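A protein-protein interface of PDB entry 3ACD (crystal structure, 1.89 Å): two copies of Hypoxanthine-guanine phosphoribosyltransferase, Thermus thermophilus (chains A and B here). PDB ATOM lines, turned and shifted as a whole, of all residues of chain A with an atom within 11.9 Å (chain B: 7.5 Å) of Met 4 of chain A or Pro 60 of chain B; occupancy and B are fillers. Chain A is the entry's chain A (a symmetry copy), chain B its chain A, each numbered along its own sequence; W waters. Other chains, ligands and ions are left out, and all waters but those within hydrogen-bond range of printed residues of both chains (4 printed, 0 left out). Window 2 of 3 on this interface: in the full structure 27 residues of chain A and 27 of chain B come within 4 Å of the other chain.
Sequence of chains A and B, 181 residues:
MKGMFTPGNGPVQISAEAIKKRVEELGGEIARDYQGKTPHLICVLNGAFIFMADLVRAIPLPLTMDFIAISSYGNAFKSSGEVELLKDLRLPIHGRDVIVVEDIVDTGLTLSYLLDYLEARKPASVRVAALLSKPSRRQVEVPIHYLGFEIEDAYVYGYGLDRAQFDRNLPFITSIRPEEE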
ATOM      1  N   MET A   4      29.048 -26.184 -19.077  1.00  0.00           N
ATOM      2  CA  MET A   4      29.573 -27.199 -20.034  1.00  0.00           C
ATOM      3  C   MET A   4      29.705 -26.634 -21.442  1.00  0.00           C
ATOM      4  O   MET A   4      29.719 -27.387 -22.416  1.00  0.00           O
ATOM      5  CB  MET A   4      28.653 -28.424 -20.068  1.00  0.00           C
ATOM      6  CG  MET A   4      28.540 -29.175 -18.752  1.00  0.00           C
ATOM      7  SD  MET A   4      27.769 -28.209 -17.443  1.00  0.00           S
ATOM      8  CE  MET A   4      29.208 -27.685 -16.508  1.00  0.00           C
ATOM      9  N   PHE A   5      29.795 -25.311 -21.555  1.00  0.00           N
ATOM     10  CA  PHE A   5      29.934 -24.683 -22.868  1.00  0.00           C
ATOM     11  C   PHE A   5      31.264 -25.109 -23.479  1.00  0.00           C
ATOM     12  O   PHE A   5      32.325 -24.778 -22.958  1.00  0.00           O
ATOM     13  CB  PHE A   5      29.879 -23.155 -22.746  1.00  0.00           C
ATOM     14  CG  PHE A   5      28.561 -22.629 -22.239  1.00  0.00           C
ATOM     15  CD1 PHE A   5      27.375 -22.939 -22.896  1.00  0.00           C
ATOM     16  CD2 PHE A   5      28.507 -21.821 -21.107  1.00  0.00           C
ATOM     17  CE1 PHE A   5      26.149 -22.452 -22.435  1.00  0.00           C
ATOM     18  CE2 PHE A   5      27.290 -21.328 -20.637  1.00  0.00           C
ATOM     19  CZ  PHE A   5      26.107 -21.647 -21.304  1.00  0.00           C
ATOM     20  N   THR A   6      31.201 -25.848 -24.582  1.00  0.00           N
ATOM     21  CA  THR A   6      32.408 -26.326 -25.246  1.00  0.00           C
ATOM     22  C   THR A   6      32.518 -25.837 -26.688  1.00  0.00           C
ATOM     23  O   THR A   6      31.560 -25.907 -27.455  1.00  0.00           O
ATOM     24  CB  THR A   6      32.467 -27.871 -25.247  1.00  0.00           C
ATOM     25  OG1 THR A   6      33.631 -28.305 -25.960  1.00  0.00           O
ATOM     26  CG2 THR A   6      31.231 -28.453 -25.913  1.00  0.00           C
ATOM     27  N   PRO A   7      33.700 -25.331 -27.070  1.00  0.00           N
ATOM     28  CA  PRO A   7      33.950 -24.823 -28.423  1.00  0.00           C
ATOM     29  C   PRO A   7      33.991 -25.941 -29.463  1.00  0.00           C
ATOM     30  O   PRO A   7      34.344 -27.082 -29.149  1.00  0.00           O
ATOM     31  CB  PRO A   7      35.310 -24.135 -28.292  1.00  0.00           C
ATOM     32  CG  PRO A   7      35.386 -23.777 -26.836  1.00  0.00           C
ATOM     33  CD  PRO A   7      34.826 -25.003 -26.181  1.00  0.00           C
ATOM     34  N   GLY A   8      33.621 -25.608 -30.695  1.00  0.00           N
ATOM     35  CA  GLY A   8      33.667 -26.586 -31.766  1.00  0.00           C
ATOM     36  C   GLY A   8      35.109 -26.617 -32.234  1.00  0.00           C
ATOM     37  O   GLY A   8      35.936 -25.878 -31.699  1.00  0.00           O
ATOM     38  N   ILE A  50      21.113 -11.515 -29.073  1.00  0.00           N
ATOM     39  CA  ILE A  50      22.075 -11.358 -27.982  1.00  0.00           C
ATOM     40  C   ILE A  50      22.998 -10.174 -28.287  1.00  0.00           C
ATOM     41  O   ILE A  50      23.296  -9.361 -27.407  1.00  0.00           O
ATOM     42  CB  ILE A  50      22.874 -12.675 -27.752  1.00  0.00           C
ATOM     43  CG1 ILE A  50      21.898 -13.764 -27.279  1.00  0.00           C
ATOM     44  CG2 ILE A  50      23.975 -12.458 -26.716  1.00  0.00           C
ATOM     45  CD1 ILE A  50      22.538 -15.062 -26.805  1.00  0.00           C
ATOM     46  N   TYR A 157      28.694 -20.367 -34.866  1.00  0.00           N
ATOM     47  CA  TYR A 157      27.505 -20.465 -34.036  1.00  0.00           C
ATOM     48  C   TYR A 157      27.830 -20.016 -32.619  1.00  0.00           C
ATOM     49  O   TYR A 157      28.999 -19.830 -32.273  1.00  0.00           O
ATOM     50  CB  TYR A 157      26.936 -21.894 -34.067  1.00  0.00           C
ATOM     51  CG  TYR A 157      27.865 -22.974 -33.560  1.00  0.00           C
ATOM     52  CD1 TYR A 157      27.814 -23.399 -32.234  1.00  0.00           C
ATOM     53  CD2 TYR A 157      28.789 -23.582 -34.415  1.00  0.00           C
ATOM     54  CE1 TYR A 157      28.659 -24.410 -31.770  1.00  0.00           C
ATOM     55  CE2 TYR A 157      29.639 -24.589 -33.959  1.00  0.00           C
ATOM     56  CZ  TYR A 157      29.568 -24.998 -32.635  1.00  0.00           C
ATOM     57  OH  TYR A 157      30.412 -25.988 -32.182  1.00  0.00           O
ATOM     58  N   GLY A 158      26.788 -19.821 -31.818  1.00  0.00           N
ATOM     59  CA  GLY A 158      26.962 -19.352 -30.457  1.00  0.00           C
ATOM     60  C   GLY A 158      26.605 -17.876 -30.400  1.00  0.00           C
ATOM     61  O   GLY A 158      26.435 -17.241 -31.443  1.00  0.00           O
ATOM     62  N   ARG A 163      23.013 -23.613 -34.663  1.00  0.00           N
ATOM     63  CA  ARG A 163      23.533 -24.753 -35.394  1.00  0.00           C
ATOM     64  C   ARG A 163      22.329 -25.689 -35.306  1.00  0.00           C
ATOM     65  O   ARG A 163      22.153 -26.398 -34.316  1.00  0.00           O
ATOM     66  CB  ARG A 163      24.750 -25.350 -34.682  1.00  0.00           C
ATOM     67  CG  ARG A 163      25.330 -26.558 -35.389  1.00  0.00           C
ATOM     68  CD  ARG A 163      26.699 -26.943 -34.846  1.00  0.00           C
ATOM     69  NE  ARG A 163      26.685 -27.198 -33.409  1.00  0.00           N
ATOM     70  CZ  ARG A 163      27.612 -27.908 -32.771  1.00  0.00           C
ATOM     71  NH1 ARG A 163      28.625 -28.438 -33.448  1.00  0.00           N
ATOM     72  NH2 ARG A 163      27.532 -28.089 -31.461  1.00  0.00           N
ATOM     73  N   PHE A 166      20.136 -25.199 -32.255  1.00  0.00           N
ATOM     74  CA  PHE A 166      20.833 -25.346 -30.977  1.00  0.00           C
ATOM     75  C   PHE A 166      22.041 -24.412 -30.892  1.00  0.00           C
ATOM     76  O   PHE A 166      22.396 -23.741 -31.861  1.00  0.00           O
ATOM     77  CB  PHE A 166      21.330 -26.791 -30.802  1.00  0.00           C
ATOM     78  CG  PHE A 166      20.245 -27.782 -30.490  1.00  0.00           C
ATOM     79  CD1 PHE A 166      19.868 -28.032 -29.174  1.00  0.00           C
ATOM     80  CD2 PHE A 166      19.609 -28.480 -31.515  1.00  0.00           C
ATOM     81  CE1 PHE A 166      18.872 -28.966 -28.879  1.00  0.00           C
ATOM     82  CE2 PHE A 166      18.613 -29.416 -31.231  1.00  0.00           C
ATOM     83  CZ  PHE A 166      18.244 -29.660 -29.910  1.00  0.00           C
ATOM     84  N   ASP A 167      22.647 -24.369 -29.709  1.00  0.00           N
ATOM     85  CA  ASP A 167      23.846 -23.582 -29.437  1.00  0.00           C
ATOM     86  C   ASP A 167      23.778 -22.056 -29.479  1.00  0.00           C
ATOM     87  O   ASP A 167      24.820 -21.400 -29.476  1.00  0.00           O
ATOM     88  CB  ASP A 167      24.988 -24.059 -30.343  1.00  0.00           C
ATOM     89  CG  ASP A 167      25.304 -25.530 -30.158  1.00  0.00           C
ATOM     90  OD1 ASP A 167      25.456 -25.962 -28.998  1.00  0.00           O
ATOM     91  OD2 ASP A 167      25.405 -26.253 -31.172  1.00  0.00           O
ATOM     92  N   ARG A 168      22.578 -21.483 -29.522  1.00  0.00           N
ATOM     93  CA  ARG A 168      22.461 -20.026 -29.522  1.00  0.00           C
ATOM     94  C   ARG A 168      22.885 -19.509 -28.144  1.00  0.00           C
ATOM     95  O   ARG A 168      23.266 -18.350 -28.000  1.00  0.00           O
ATOM     96  CB  ARG A 168      21.013 -19.581 -29.771  1.00  0.00           C
ATOM     97  CG  ARG A 168      20.428 -19.893 -31.148  1.00  0.00           C
ATOM     98  CD  ARG A 168      19.021 -19.294 -31.239  1.00  0.00           C
ATOM     99  NE  ARG A 168      18.273 -19.733 -32.415  1.00  0.00           N
ATOM    100  CZ  ARG A 168      18.454 -19.272 -33.649  1.00  0.00           C
ATOM    101  NH1 ARG A 168      19.368 -18.341 -33.894  1.00  0.00           N
ATOM    102  NH2 ARG A 168      17.710 -19.746 -34.642  1.00  0.00           N
ATOM    103  N   ASN A 169      22.827 -20.381 -27.137  1.00  0.00           N
ATOM    104  CA  ASN A 169      23.162 -19.994 -25.771  1.00  0.00           C
ATOM    105  C   ASN A 169      24.641 -19.964 -25.383  1.00  0.00           C
ATOM    106  O   ASN A 169      24.976 -19.567 -24.269  1.00  0.00           O
ATOM    107  CB  ASN A 169      22.369 -20.864 -24.778  1.00  0.00           C
ATOM    108  CG  ASN A 169      22.636 -22.353 -24.947  1.00  0.00           C
ATOM    109  OD1 ASN A 169      22.724 -22.861 -26.065  1.00  0.00           O
ATOM    110  ND2 ASN A 169      22.737 -23.061 -23.831  1.00  0.00           N
ATOM    111  N   LEU A 170      25.527 -20.375 -26.285  1.00  0.00           N
ATOM    112  CA  LEU A 170      26.958 -20.329 -25.988  1.00  0.00           C
ATOM    113  C   LEU A 170      27.334 -18.854 -25.834  1.00  0.00           C
ATOM    114  O   LEU A 170      26.965 -18.023 -26.665  1.00  0.00           O
ATOM    115  CB  LEU A 170      27.770 -20.969 -27.123  1.00  0.00           C
ATOM    116  CG  LEU A 170      28.055 -22.477 -27.050  1.00  0.00           C
ATOM    117  CD1 LEU A 170      26.794 -23.253 -26.720  1.00  0.00           C
ATOM    118  CD2 LEU A 170      28.646 -22.937 -28.381  1.00  0.00           C
ATOM    119  N   PRO A 171      28.061 -18.505 -24.763  1.00  0.00           N
ATOM    120  CA  PRO A 171      28.454 -17.108 -24.551  1.00  0.00           C
ATOM    121  C   PRO A 171      29.558 -16.610 -25.484  1.00  0.00           C
ATOM    122  O   PRO A 171      29.897 -15.424 -25.486  1.00  0.00           O
ATOM    123  CB  PRO A 171      28.871 -17.089 -23.081  1.00  0.00           C
ATOM    124  CG  PRO A 171      29.437 -18.459 -22.883  1.00  0.00           C
ATOM    125  CD  PRO A 171      28.451 -19.344 -23.614  1.00  0.00           C
ATOM    126  N   PHE A 172      30.103 -17.518 -26.282  1.00  0.00           N
ATOM    127  CA  PHE A 172      31.172 -17.175 -27.212  1.00  0.00           C
ATOM    128  C   PHE A 172      30.829 -17.599 -28.633  1.00  0.00           C
ATOM    129  O   PHE A 172      29.841 -18.297 -28.869  1.00  0.00           O
ATOM    130  CB  PHE A 172      32.473 -17.850 -26.767  1.00  0.00           C
ATOM    131  CG  PHE A 172      32.327 -19.326 -26.505  1.00  0.00           C
ATOM    132  CD1 PHE A 172      32.191 -20.229 -27.558  1.00  0.00           C
ATOM    133  CD2 PHE A 172      32.281 -19.810 -25.200  1.00  0.00           C
ATOM    134  CE1 PHE A 172      32.009 -21.592 -27.316  1.00  0.00           C
ATOM    135  CE2 PHE A 172      32.097 -21.172 -24.945  1.00  0.00           C
ATOM    136  CZ  PHE A 172      31.959 -22.064 -26.006  1.00  0.00           C
ATOM    137  N   THR A 174      31.940 -19.718 -31.880  1.00  0.00           N
ATOM    138  CA  THR A 174      32.789 -20.843 -32.245  1.00  0.00           C
ATOM    139  C   THR A 174      32.383 -21.318 -33.637  1.00  0.00           C
ATOM    140  O   THR A 174      31.557 -20.685 -34.296  1.00  0.00           O
ATOM    141  CB  THR A 174      32.685 -21.991 -31.209  1.00  0.00           C
ATOM    142  OG1 THR A 174      33.594 -23.042 -31.561  1.00  0.00           O
ATOM    143  CG2 THR A 174      31.280 -22.539 -31.147  1.00  0.00           C
ATOM    144  N   GLY B  27      19.756 -19.080 -13.953  1.00  0.00           N
ATOM    145  CA  GLY B  27      20.270 -19.962 -14.983  1.00  0.00           C
ATOM    146  C   GLY B  27      20.813 -21.239 -14.363  1.00  0.00           C
ATOM    147  O   GLY B  27      20.621 -22.332 -14.894  1.00  0.00           O
ATOM    148  N   GLY B  28      21.496 -21.095 -13.233  1.00  0.00           N
ATOM    149  CA  GLY B  28      22.050 -22.251 -12.551  1.00  0.00           C
ATOM    150  C   GLY B  28      20.959 -23.187 -12.069  1.00  0.00           C
ATOM    151  O   GLY B  28      21.087 -24.408 -12.185  1.00  0.00           O
ATOM    152  N   ILE B  30      17.928 -23.508 -13.308  1.00  0.00           N
ATOM    153  CA  ILE B  30      17.328 -24.140 -14.475  1.00  0.00           C
ATOM    154  C   ILE B  30      18.199 -25.288 -14.977  1.00  0.00           C
ATOM    155  O   ILE B  30      17.698 -26.371 -15.275  1.00  0.00           O
ATOM    156  CB  ILE B  30      17.114 -23.106 -15.612  1.00  0.00           C
ATOM    157  CG1 ILE B  30      16.013 -22.123 -15.204  1.00  0.00           C
ATOM    158  CG2 ILE B  30      16.744 -23.815 -16.914  1.00  0.00           C
ATOM    159  CD1 ILE B  30      15.835 -20.946 -16.142  1.00  0.00           C
ATOM    160  N   ALA B  31      19.504 -25.050 -15.058  1.00  0.00           N
ATOM    161  CA  ALA B  31      20.437 -26.068 -15.530  1.00  0.00           C
ATOM    162  C   ALA B  31      20.355 -27.312 -14.646  1.00  0.00           C
ATOM    163  O   ALA B  31      20.378 -28.441 -15.137  1.00  0.00           O
ATOM    164  CB  ALA B  31      21.855 -25.512 -15.533  1.00  0.00           C
ATOM    165  N   ARG B  32      20.250 -27.093 -13.341  1.00  0.00           N
ATOM    166  CA  ARG B  32      20.153 -28.191 -12.384  1.00  0.00           C
ATOM    167  C   ARG B  32      18.817 -28.915 -12.515  1.00  0.00           C
ATOM    168  O   ARG B  32      18.773 -30.144 -12.587  1.00  0.00           O
ATOM    169  CB  ARG B  32      20.302 -27.667 -10.953  1.00  0.00           C
ATOM    170  CG  ARG B  32      20.083 -28.730  -9.886  1.00  0.00           C
ATOM    171  CD  ARG B  32      20.073 -28.141  -8.485  1.00  0.00           C
ATOM    172  NE  ARG B  32      21.355 -27.540  -8.126  1.00  0.00           N
ATOM    173  CZ  ARG B  32      21.628 -27.025  -6.931  1.00  0.00           C
ATOM    174  NH1 ARG B  32      20.709 -27.039  -5.975  1.00  0.00           N
ATOM    175  NH2 ARG B  32      22.821 -26.496  -6.691  1.00  0.00           N
ATOM    176  N   LEU B  55      19.970 -14.736 -19.538  1.00  0.00           N
ATOM    177  CA  LEU B  55      19.566 -16.006 -18.945  1.00  0.00           C
ATOM    178  C   LEU B  55      20.079 -17.236 -19.698  1.00  0.00           C
ATOM    179  O   LEU B  55      20.640 -18.146 -19.086  1.00  0.00           O
ATOM    180  CB  LEU B  55      18.033 -16.084 -18.841  1.00  0.00           C
ATOM    181  CG  LEU B  55      17.467 -17.358 -18.195  1.00  0.00           C
ATOM    182  CD1 LEU B  55      17.906 -17.430 -16.744  1.00  0.00           C
ATOM    183  CD2 LEU B  55      15.944 -17.365 -18.281  1.00  0.00           C
ATOM    184  N   VAL B  56      19.895 -17.278 -21.018  1.00  0.00           N
ATOM    185  CA  VAL B  56      20.340 -18.445 -21.770  1.00  0.00           C
ATOM    186  C   VAL B  56      21.848 -18.666 -21.677  1.00  0.00           C
ATOM    187  O   VAL B  56      22.311 -19.807 -21.656  1.00  0.00           O
ATOM    188  CB  VAL B  56      19.900 -18.384 -23.262  1.00  0.00           C
ATOM    189  CG1 VAL B  56      18.377 -18.317 -23.342  1.00  0.00           C
ATOM    190  CG2 VAL B  56      20.540 -17.195 -23.973  1.00  0.00           C
ATOM    191  N   ARG B  57      22.610 -17.581 -21.592  1.00  0.00           N
ATOM    192  CA  ARG B  57      24.058 -17.694 -21.485  1.00  0.00           C
ATOM    193  C   ARG B  57      24.488 -18.213 -20.117  1.00  0.00           C
ATOM    194  O   ARG B  57      25.675 -18.449 -19.883  1.00  0.00           O
ATOM    195  CB  ARG B  57      24.719 -16.345 -21.770  1.00  0.00           C
ATOM    196  CG  ARG B  57      24.756 -16.008 -23.256  1.00  0.00           C
ATOM    197  CD  ARG B  57      25.417 -14.669 -23.516  1.00  0.00           C
ATOM    198  NE  ARG B  57      24.557 -13.543 -23.159  1.00  0.00           N
ATOM    199  CZ  ARG B  57      24.877 -12.272 -23.387  1.00  0.00           C
ATOM    200  NH1 ARG B  57      26.036 -11.984 -23.968  1.00  0.00           N
ATOM    201  NH2 ARG B  57      24.040 -11.293 -23.053  1.00  0.00           N
ATOM    202  N   ALA B  58      23.517 -18.394 -19.222  1.00  0.00           N
ATOM    203  CA  ALA B  58      23.794 -18.912 -17.882  1.00  0.00           C
ATOM    204  C   ALA B  58      23.169 -20.298 -17.714  1.00  0.00           C
ATOM    205  O   ALA B  58      23.043 -20.804 -16.601  1.00  0.00           O
ATOM    206  CB  ALA B  58      23.251 -17.959 -16.822  1.00  0.00           C
ATOM    207  N   ILE B  59      22.774 -20.908 -18.829  1.00  0.00           N
ATOM    208  CA  ILE B  59      22.181 -22.241 -18.803  1.00  0.00           C
ATOM    209  C   ILE B  59      23.008 -23.180 -19.681  1.00  0.00           C
ATOM    210  O   ILE B  59      22.771 -23.295 -20.886  1.00  0.00           O
ATOM    211  CB  ILE B  59      20.733 -22.240 -19.332  1.00  0.00           C
ATOM    212  CG1 ILE B  59      19.861 -21.311 -18.484  1.00  0.00           C
ATOM    213  CG2 ILE B  59      20.165 -23.659 -19.290  1.00  0.00           C
ATOM    214  CD1 ILE B  59      18.459 -21.131 -19.034  1.00  0.00           C
ATOM    215  N   PRO B  60      24.001 -23.856 -19.086  1.00  0.00           N
ATOM    216  CA  PRO B  60      24.847 -24.779 -19.847  1.00  0.00           C
ATOM    217  C   PRO B  60      24.170 -26.121 -20.115  1.00  0.00           C
ATOM    218  O   PRO B  60      24.519 -27.141 -19.519  1.00  0.00           O
ATOM    219  CB  PRO B  60      26.090 -24.905 -18.968  1.00  0.00           C
ATOM    220  CG  PRO B  60      25.529 -24.791 -17.595  1.00  0.00           C
ATOM    221  CD  PRO B  60      24.533 -23.657 -17.726  1.00  0.00           C
ATOM    222  N   LEU B  61      23.197 -26.096 -21.023  1.00  0.00           N
ATOM    223  CA  LEU B  61      22.442 -27.276 -21.434  1.00  0.00           C
ATOM    224  C   LEU B  61      22.101 -27.119 -22.909  1.00  0.00           C
ATOM    225  O   LEU B  61      22.100 -26.005 -23.432  1.00  0.00           O
ATOM    226  CB  LEU B  61      21.119 -27.376 -20.667  1.00  0.00           C
ATOM    227  CG  LEU B  61      21.087 -27.750 -19.188  1.00  0.00           C
ATOM    228  CD1 LEU B  61      19.651 -27.639 -18.679  1.00  0.00           C
ATOM    229  CD2 LEU B  61      21.609 -29.166 -19.006  1.00  0.00           C
ATOM    230  N   PRO B  62      21.828 -28.233 -23.607  1.00  0.00           N
ATOM    231  CA  PRO B  62      21.478 -28.106 -25.023  1.00  0.00           C
ATOM    232  C   PRO B  62      20.034 -27.619 -25.005  1.00  0.00           C
ATOM    233  O   PRO B  62      19.196 -28.178 -24.297  1.00  0.00           O
ATOM    234  CB  PRO B  62      21.606 -29.534 -25.537  1.00  0.00           C
ATOM    235  CG  PRO B  62      21.177 -30.346 -24.347  1.00  0.00           C
ATOM    236  CD  PRO B  62      21.888 -29.650 -23.202  1.00  0.00           C
ATOM    237  N   LEU B  63      19.738 -26.566 -25.754  1.00  0.00           N
ATOM    238  CA  LEU B  63      18.384 -26.037 -25.755  1.00  0.00           C
ATOM    239  C   LEU B  63      18.069 -25.288 -27.034  1.00  0.00           C
ATOM    240  O   LEU B  63      18.975 -24.889 -27.768  1.00  0.00           O
ATOM    241  CB  LEU B  63      18.198 -25.112 -24.545  1.00  0.00           C
ATOM    242  CG  LEU B  63      19.177 -23.938 -24.384  1.00  0.00           C
ATOM    243  CD1 LEU B  63      18.777 -22.784 -25.297  1.00  0.00           C
ATOM    244  CD2 LEU B  63      19.165 -23.469 -22.930  1.00  0.00           C
HETATM  245  O   HOH W   1      22.150 -25.377 -27.019  1.00  0.00           O
HETATM  246  O   HOH W   2      19.774 -22.645 -29.142  1.00  0.00           O
HETATM  247  O   HOH W   3      24.696 -28.287 -17.121  1.00  0.00           O
HETATM  248  O   HOH W   4      28.649 -13.573 -24.060  1.00  0.00           O
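Of the 14 printed residues of chain B, 6 touch a printed residue of chain A. Hydrophobic or aromatic side chains of chain A that line the printed part of chain B: Phe 5, Ile 50 and Phe 166. Among the printed residues, no Asp or Glu carboxylate lies within 4 Å of a Lys or Arg side-chain nitrogen of the other chain.
Printed residues of chain B within 4 Å of Phe 5 of chain A: Arg 57, Ile 59 and Pro 60. Of the printed residues of chain B, Ile 50 of chain A touches Arg 57. Printed residues of chain B within 4 Å of Asn 169 of chain A: Val 56 (3.3 Å), Arg 57 (3.5 Å), Ile 59 (3.0 Å), Leu 61 (3.0 Å) and Leu 63 (3.7 Å). No residue of chain A comes within 4 Å of Gly 27 of chain B. No residue of chain A comes within 4 Å of Gly 28 of chain B. Ile 59 of chain B touches just these residues of chain A: Phe 5 (3.7 Å) and Asn 169 (3.0 Å). Pro 60 of chain B touches two residues of chain A. Of the printed residues of chain A, Leu 61 of chain B touches Asn 169. Printed residues of chain A within 4 Å of Leu 63 of chain B: Phe 166 and Asn 169. The nearest residue of chain A that does not touch Pro 60 of chain B is Asn 169 of chain A (4.8 Å).
Among the printed residues, merely in contact across the chains: Met 4 of chain A with Pro 60 of chain B (3.2 Å), Phe 5 of chain A with Arg 57 of chain B (3.4 Å), Phe 5 of chain A with Ile 59 of chain B (3.7 Å), Phe 5 of chain A with Pro 60 of chain B (3.7 Å), Ile 50 of chain A with Arg 57 of chain B (3.5 Å), Phe 166 of chain A with Leu 63 of chain B (3.6 Å), Asn 169 of chain A with Val 56 of chain B (3.3 Å), Asn 169 of chain A with Arg 57 of chain B (3.5 Å) and Asn 169 of chain A with Leu 63 of chain B (3.7 Å).
No position is printed for both chains.
Water W4 lies within hydrogen-bond range of the backbone carbonyl oxygen of Pro 171 of chain A and the guanidinium group of Arg 57 of chain B. Water W3 bridges the backbone carbonyl oxygen (O) of Pro 60 of chain B (2.7 Å) and the side-chain sulfur (SD) of Met 4 of chain A (3.1 Å). Water W2 lies within hydrogen-bond range of the backbone carbonyl oxygen (O) of Leu 63 of chain B (2.7 Å), the backbone NH (N) of Arg 168 of chain A (3.1 Å) and the backbone NH (N) of Asp 167 of chain A (3.4 Å). Water W1 lies within hydrogen-bond range of the side-chain amide oxygen of Asn 169 of chain A, the backbone NH of Asp 167 of chain A and the backbone NH of Leu 63 of chain B.
The side-chain amide nitrogen of Asn 169 of chain A lies within hydrogen-bond range of the backbone carbonyl oxygen of Ile 59 of chain B (3.0 Å). The backbone carbonyl oxygen (O) of Leu 61 of chain B sits at hydrogen-bond distance from the side-chain amide nitrogen (ND2) of Asn 169 of chain A (3.0 Å).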
